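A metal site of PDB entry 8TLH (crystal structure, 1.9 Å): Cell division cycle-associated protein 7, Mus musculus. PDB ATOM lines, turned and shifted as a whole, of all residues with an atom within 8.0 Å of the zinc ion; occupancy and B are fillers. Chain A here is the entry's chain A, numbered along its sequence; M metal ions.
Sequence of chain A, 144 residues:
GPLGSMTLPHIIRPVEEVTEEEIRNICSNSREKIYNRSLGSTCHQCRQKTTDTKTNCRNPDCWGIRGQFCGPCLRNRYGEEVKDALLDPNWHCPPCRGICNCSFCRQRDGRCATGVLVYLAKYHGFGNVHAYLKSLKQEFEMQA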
ATOM      1  N   HIS A  10       6.765   6.643  29.759  1.00  0.00           N
ATOM      2  CA  HIS A  10       5.730   7.345  29.036  1.00  0.00           C
ATOM      3  C   HIS A  10       4.486   6.468  28.955  1.00  0.00           C
ATOM      4  O   HIS A  10       4.541   5.354  28.436  1.00  0.00           O
ATOM      5  CB  HIS A  10       6.213   7.715  27.636  1.00  0.00           C
ATOM      6  CG  HIS A  10       5.159   8.316  26.773  1.00  0.00           C
ATOM      7  ND1 HIS A  10       4.752   7.750  25.585  1.00  0.00           N
ATOM      8  CD2 HIS A  10       4.412   9.435  26.920  1.00  0.00           C
ATOM      9  CE1 HIS A  10       3.807   8.496  25.039  1.00  0.00           C
ATOM     10  NE2 HIS A  10       3.579   9.529  25.834  1.00  0.00           N
ATOM     11  N   ASN A  56      -0.579  15.044  26.935  1.00  0.00           N
ATOM     12  CA  ASN A  56      -0.091  13.675  26.906  1.00  0.00           C
ATOM     13  C   ASN A  56       0.082  13.261  25.453  1.00  0.00           C
ATOM     14  O   ASN A  56      -0.898  13.115  24.723  1.00  0.00           O
ATOM     15  CB  ASN A  56      -1.047  12.729  27.632  1.00  0.00           C
ATOM     16  CG  ASN A  56      -0.671  11.266  27.467  1.00  0.00           C
ATOM     17  OD1 ASN A  56      -1.325  10.531  26.722  1.00  0.00           O
ATOM     18  ND2 ASN A  56       0.374  10.834  28.162  1.00  0.00           N
ATOM     19  N   CYS A  57       1.334  13.096  25.020  1.00  0.00           N
ATOM     20  CA  CYS A  57       1.608  12.684  23.649  1.00  0.00           C
ATOM     21  C   CYS A  57       1.170  11.245  23.445  1.00  0.00           C
ATOM     22  O   CYS A  57       1.455  10.369  24.269  1.00  0.00           O
ATOM     23  CB  CYS A  57       3.092  12.843  23.326  1.00  0.00           C
ATOM     24  SG  CYS A  57       3.546  12.432  21.622  1.00  0.00           S
ATOM     25  N   ARG A  58       0.462  10.994  22.345  1.00  0.00           N
ATOM     26  CA  ARG A  58      -0.070   9.666  22.054  1.00  0.00           C
ATOM     27  C   ARG A  58       0.705   8.957  20.954  1.00  0.00           C
ATOM     28  O   ARG A  58       0.217   7.966  20.397  1.00  0.00           O
ATOM     29  CB  ARG A  58      -1.555   9.763  21.705  1.00  0.00           C
ATOM     30  CG  ARG A  58      -2.369  10.331  22.849  1.00  0.00           C
ATOM     31  CD  ARG A  58      -3.862  10.246  22.625  1.00  0.00           C
ATOM     32  NE  ARG A  58      -4.589  10.602  23.844  1.00  0.00           N
ATOM     33  CZ  ARG A  58      -4.893  11.840  24.203  1.00  0.00           C
ATOM     34  NH1 ARG A  58      -4.568  12.879  23.444  1.00  0.00           N
ATOM     35  NH2 ARG A  58      -5.523  12.045  25.357  1.00  0.00           N
ATOM     36  N   ASN A  59       1.898   9.442  20.622  1.00  0.00           N
ATOM     37  CA  ASN A  59       2.786   8.708  19.729  1.00  0.00           C
ATOM     38  C   ASN A  59       3.459   7.577  20.499  1.00  0.00           C
ATOM     39  O   ASN A  59       4.119   7.842  21.503  1.00  0.00           O
ATOM     40  CB  ASN A  59       3.843   9.644  19.148  1.00  0.00           C
ATOM     41  CG  ASN A  59       4.807   8.946  18.206  1.00  0.00           C
ATOM     42  OD1 ASN A  59       4.516   7.867  17.692  1.00  0.00           O
ATOM     43  ND2 ASN A  59       5.961   9.554  17.980  1.00  0.00           N
ATOM     44  N   PRO A  60       3.304   6.323  20.070  1.00  0.00           N
ATOM     45  CA  PRO A  60       3.937   5.223  20.812  1.00  0.00           C
ATOM     46  C   PRO A  60       5.451   5.329  20.886  1.00  0.00           C
ATOM     47  O   PRO A  60       6.061   4.795  21.819  1.00  0.00           O
ATOM     48  CB  PRO A  60       3.488   3.977  20.038  1.00  0.00           C
ATOM     49  CG  PRO A  60       2.232   4.392  19.354  1.00  0.00           C
ATOM     50  CD  PRO A  60       2.438   5.833  18.991  1.00  0.00           C
ATOM     51  N   ASP A  61       6.084   6.002  19.930  1.00  0.00           N
ATOM     52  CA  ASP A  61       7.536   6.144  19.921  1.00  0.00           C
ATOM     53  C   ASP A  61       8.025   7.290  20.799  1.00  0.00           C
ATOM     54  O   ASP A  61       9.241   7.447  20.970  1.00  0.00           O
ATOM     55  CB  ASP A  61       8.040   6.337  18.487  1.00  0.00           C
ATOM     56  CG  ASP A  61       9.526   6.079  18.349  1.00  0.00           C
ATOM     57  OD1 ASP A  61       9.959   4.918  18.557  1.00  0.00           O
ATOM     58  OD2 ASP A  61      10.270   7.037  18.057  1.00  0.00           O
ATOM     59  N   CYS A  62       7.120   8.088  21.359  1.00  0.00           N
ATOM     60  CA  CYS A  62       7.516   9.137  22.285  1.00  0.00           C
ATOM     61  C   CYS A  62       7.995   8.516  23.594  1.00  0.00           C
ATOM     62  O   CYS A  62       7.682   7.380  23.925  1.00  0.00           O
ATOM     63  CB  CYS A  62       6.340  10.089  22.540  1.00  0.00           C
ATOM     64  SG  CYS A  62       6.818  11.724  23.147  1.00  0.00           S
ATOM     65  N   TRP A  63       8.777   9.291  24.340  1.00  0.00           N
ATOM     66  CA  TRP A  63       9.354   8.818  25.585  1.00  0.00           C
ATOM     67  C   TRP A  63       9.542   9.989  26.533  1.00  0.00           C
ATOM     68  O   TRP A  63       9.667  11.139  26.116  1.00  0.00           O
ATOM     69  CB  TRP A  63      10.696   8.107  25.357  1.00  0.00           C
ATOM     70  CG  TRP A  63      11.803   9.049  25.000  1.00  0.00           C
ATOM     71  CD1 TRP A  63      12.776   9.526  25.829  1.00  0.00           C
ATOM     72  CD2 TRP A  63      12.048   9.648  23.719  1.00  0.00           C
ATOM     73  NE1 TRP A  63      13.616  10.374  25.149  1.00  0.00           N
ATOM     74  CE2 TRP A  63      13.193  10.465  23.845  1.00  0.00           C
ATOM     75  CE3 TRP A  63      11.416   9.566  22.475  1.00  0.00           C
ATOM     76  CZ2 TRP A  63      13.715  11.198  22.783  1.00  0.00           C
ATOM     77  CZ3 TRP A  63      11.938  10.293  21.421  1.00  0.00           C
ATOM     78  CH2 TRP A  63      13.070  11.099  21.575  1.00  0.00           C
ATOM     79  N   GLY A  64       9.583   9.671  27.830  1.00  0.00           N
ATOM     80  CA  GLY A  64       9.894  10.666  28.827  1.00  0.00           C
ATOM     81  C   GLY A  64       8.821  11.740  28.957  1.00  0.00           C
ATOM     82  O   GLY A  64       7.629  11.507  28.742  1.00  0.00           O
ATOM     83  N   ILE A  65       9.269  12.941  29.312  1.00  0.00           N
ATOM     84  CA  ILE A  65       8.373  14.070  29.578  1.00  0.00           C
ATOM     85  C   ILE A  65       8.343  15.059  28.418  1.00  0.00           C
ATOM     86  O   ILE A  65       7.732  16.126  28.524  1.00  0.00           O
ATOM     87  CB  ILE A  65       8.754  14.774  30.882  1.00  0.00           C
ATOM     88  CG1 ILE A  65      10.098  15.468  30.730  1.00  0.00           C
ATOM     89  CG2 ILE A  65       8.807  13.776  32.014  1.00  0.00           C
ATOM     90  CD1 ILE A  65      10.246  16.710  31.580  1.00  0.00           C
ATOM     91  N   ARG A  66       9.005  14.736  27.299  1.00  0.00           N
ATOM     92  CA  ARG A  66       9.105  15.666  26.175  1.00  0.00           C
ATOM     93  C   ARG A  66       7.754  16.032  25.590  1.00  0.00           C
ATOM     94  O   ARG A  66       7.630  17.077  24.935  1.00  0.00           O
ATOM     95  CB  ARG A  66      10.007  15.093  25.086  1.00  0.00           C
ATOM     96  CG  ARG A  66       9.453  13.863  24.378  1.00  0.00           C
ATOM     97  CD  ARG A  66      10.557  13.029  23.728  1.00  0.00           C
ATOM     98  NE  ARG A  66      11.122  13.684  22.552  1.00  0.00           N
ATOM     99  CZ  ARG A  66      10.634  13.572  21.327  1.00  0.00           C
ATOM    100  NH1 ARG A  66       9.565  12.831  21.083  1.00  0.00           N
ATOM    101  NH2 ARG A  66      11.210  14.221  20.332  1.00  0.00           N
ATOM    102  N   GLY A  67       6.737  15.201  25.804  1.00  0.00           N
ATOM    103  CA  GLY A  67       5.391  15.451  25.313  1.00  0.00           C
ATOM    104  C   GLY A  67       4.480  16.207  26.254  1.00  0.00           C
ATOM    105  O   GLY A  67       3.293  16.375  25.936  1.00  0.00           O
ATOM    106  N   GLN A  68       4.974  16.690  27.383  1.00  0.00           N
ATOM    107  CA  GLN A  68       4.152  17.364  28.381  1.00  0.00           C
ATOM    108  C   GLN A  68       4.304  18.873  28.230  1.00  0.00           C
ATOM    109  O   GLN A  68       5.404  19.418  28.394  1.00  0.00           O
ATOM    110  CB  GLN A  68       4.551  16.932  29.799  1.00  0.00           C
ATOM    111  CG  GLN A  68       4.492  15.425  30.021  1.00  0.00           C
ATOM    112  CD  GLN A  68       4.967  15.023  31.400  1.00  0.00           C
ATOM    113  OE1 GLN A  68       5.349  15.866  32.217  1.00  0.00           O
ATOM    114  NE2 GLN A  68       4.948  13.721  31.672  1.00  0.00           N
ATOM    115  N   PHE A  69       3.195  19.552  27.944  1.00  0.00           N
ATOM    116  CA  PHE A  69       3.170  20.995  27.765  1.00  0.00           C
ATOM    117  C   PHE A  69       2.048  21.589  28.587  1.00  0.00           C
ATOM    118  O   PHE A  69       0.936  21.051  28.623  1.00  0.00           O
ATOM    119  CB  PHE A  69       2.992  21.375  26.284  1.00  0.00           C
ATOM    120  CG  PHE A  69       4.208  21.114  25.437  1.00  0.00           C
ATOM    121  CD1 PHE A  69       4.492  19.839  24.964  1.00  0.00           C
ATOM    122  CD2 PHE A  69       5.076  22.149  25.098  1.00  0.00           C
ATOM    123  CE1 PHE A  69       5.608  19.605  24.190  1.00  0.00           C
ATOM    124  CE2 PHE A  69       6.192  21.916  24.324  1.00  0.00           C
ATOM    125  CZ  PHE A  69       6.463  20.634  23.870  1.00  0.00           C
ATOM    126  N   TRP A  91      -3.082  13.121  18.751  1.00  0.00           N
ATOM    127  CA  TRP A  91      -2.212  14.253  19.035  1.00  0.00           C
ATOM    128  C   TRP A  91      -0.774  13.798  19.279  1.00  0.00           C
ATOM    129  O   TRP A  91      -0.532  12.873  20.051  1.00  0.00           O
ATOM    130  CB  TRP A  91      -2.720  15.037  20.238  1.00  0.00           C
ATOM    131  CG  TRP A  91      -2.003  16.327  20.451  1.00  0.00           C
ATOM    132  CD1 TRP A  91      -2.228  17.513  19.808  1.00  0.00           C
ATOM    133  CD2 TRP A  91      -0.912  16.572  21.354  1.00  0.00           C
ATOM    134  NE1 TRP A  91      -1.358  18.472  20.257  1.00  0.00           N
ATOM    135  CE2 TRP A  91      -0.543  17.924  21.206  1.00  0.00           C
ATOM    136  CE3 TRP A  91      -0.227  15.779  22.275  1.00  0.00           C
ATOM    137  CZ2 TRP A  91       0.489  18.502  21.944  1.00  0.00           C
ATOM    138  CZ3 TRP A  91       0.800  16.345  23.006  1.00  0.00           C
ATOM    139  CH2 TRP A  91       1.151  17.693  22.844  1.00  0.00           C
ATOM    140  N   HIS A  92       0.163  14.454  18.605  1.00  0.00           N
ATOM    141  CA  HIS A  92       1.594  14.241  18.805  1.00  0.00           C
ATOM    142  C   HIS A  92       2.217  15.534  19.320  1.00  0.00           C
ATOM    143  O   HIS A  92       1.811  16.626  18.921  1.00  0.00           O
ATOM    144  CB  HIS A  92       2.283  13.819  17.502  1.00  0.00           C
ATOM    145  CG  HIS A  92       1.942  12.432  17.063  1.00  0.00           C
ATOM    146  ND1 HIS A  92       2.598  11.801  16.019  1.00  0.00           N
ATOM    147  CD2 HIS A  92       1.030  11.548  17.524  1.00  0.00           C
ATOM    148  CE1 HIS A  92       2.090  10.595  15.857  1.00  0.00           C
ATOM    149  NE2 HIS A  92       1.143  10.409  16.747  1.00  0.00           N
ATOM    150  N   CYS A  93       3.202  15.397  20.208  1.00  0.00           N
ATOM    151  CA  CYS A  93       3.839  16.579  20.773  1.00  0.00           C
ATOM    152  C   CYS A  93       4.701  17.279  19.718  1.00  0.00           C
ATOM    153  O   CYS A  93       5.101  16.660  18.726  1.00  0.00           O
ATOM    154  CB  CYS A  93       4.688  16.200  21.983  1.00  0.00           C
ATOM    155  SG  CYS A  93       6.125  15.161  21.657  1.00  0.00           S
ATOM    156  N   PRO A  94       4.954  18.565  19.901  1.00  0.00           N
ATOM    157  CA  PRO A  94       5.791  19.312  18.943  1.00  0.00           C
ATOM    158  C   PRO A  94       7.171  18.681  18.773  1.00  0.00           C
ATOM    159  O   PRO A  94       7.695  18.669  17.649  1.00  0.00           O
ATOM    160  CB  PRO A  94       5.874  20.713  19.562  1.00  0.00           C
ATOM    161  CG  PRO A  94       4.603  20.852  20.314  1.00  0.00           C
ATOM    162  CD  PRO A  94       4.287  19.476  20.853  1.00  0.00           C
ATOM    163  N   PRO A  95       7.805  18.168  19.833  1.00  0.00           N
ATOM    164  CA  PRO A  95       9.054  17.415  19.603  1.00  0.00           C
ATOM    165  C   PRO A  95       8.870  16.226  18.667  1.00  0.00           C
ATOM    166  O   PRO A  95       9.742  15.971  17.832  1.00  0.00           O
ATOM    167  CB  PRO A  95       9.462  16.967  21.012  1.00  0.00           C
ATOM    168  CG  PRO A  95       8.937  18.037  21.884  1.00  0.00           C
ATOM    169  CD  PRO A  95       7.617  18.422  21.275  1.00  0.00           C
ATOM    170  N   CYS A  96       7.769  15.491  18.786  1.00  0.00           N
ATOM    171  CA  CYS A  96       7.508  14.395  17.857  1.00  0.00           C
ATOM    172  C   CYS A  96       7.269  14.918  16.448  1.00  0.00           C
ATOM    173  O   CYS A  96       7.700  14.303  15.458  1.00  0.00           O
ATOM    174  CB  CYS A  96       6.308  13.567  18.326  1.00  0.00           C
ATOM    175  SG  CYS A  96       6.726  12.291  19.531  1.00  0.00           S
ATOM    176  N   ARG A  97       6.576  16.054  16.327  1.00  0.00           N
ATOM    177  CA  ARG A  97       6.351  16.677  15.033  1.00  0.00           C
ATOM    178  C   ARG A  97       7.580  17.400  14.504  1.00  0.00           C
ATOM    179  O   ARG A  97       7.561  17.855  13.357  1.00  0.00           O
ATOM    180  CB  ARG A  97       5.169  17.643  15.122  1.00  0.00           C
ATOM    181  CG  ARG A  97       3.809  16.963  15.143  1.00  0.00           C
ATOM    182  CD  ARG A  97       2.684  17.969  15.291  1.00  0.00           C
ATOM    183  NE  ARG A  97       2.455  18.343  16.686  1.00  0.00           N
ATOM    184  CZ  ARG A  97       1.626  19.294  17.082  1.00  0.00           C
ATOM    185  NH1 ARG A  97       0.928  20.013  16.209  1.00  0.00           N
ATOM    186  NH2 ARG A  97       1.486  19.532  18.376  1.00  0.00           N
HETATM  187 ZN    ZN M   1       5.777  12.902  21.567  1.00  0.00          ZN
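The side-chain sulfur (SG) of Cys 62 lies close to the guanidinium group (NH1) of Arg 66, at 3.6 Å.
The backbone carbonyl oxygen (O) of Cys 62 lies within hydrogen-bond range of a ring nitrogen (ND1) of His 10, 3.4 Å away.
The side-chain sulfur of Cys 57 sits close to the backbone NH of Asn 59, at 3.6 Å.
O of Cys 57 sits at hydrogen-bond distance from NE2 of His 10 (2.8 Å).
The side-chain sulfur of Cys 96 sits close to the guanidinium group of Arg 66, 3.3 Å away.
The side-chain sulfur (SG) of Cys 96 lies close to the side-chain amide nitrogen (ND2) of Asn 59 (3.2 Å).
O of Pro 95 sits close to NH2 of Arg 66 (3.4 Å).
Arg 66 touches the zinc ion (NH1 to ZN, 3.8 Å).
The nearest printed residue that does not touch the zinc ion is Asn 59 (4.5 Å).
The zinc ion is bound by the side-chain sulfur (SG) of Cys 62 (2.2 Å), the side-chain sulfur (SG) of Cys 57 (2.3 Å), the side-chain sulfur (SG) of Cys 93 (2.3 Å) and the side-chain sulfur (SG) of Cys 96 (2.3 Å).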
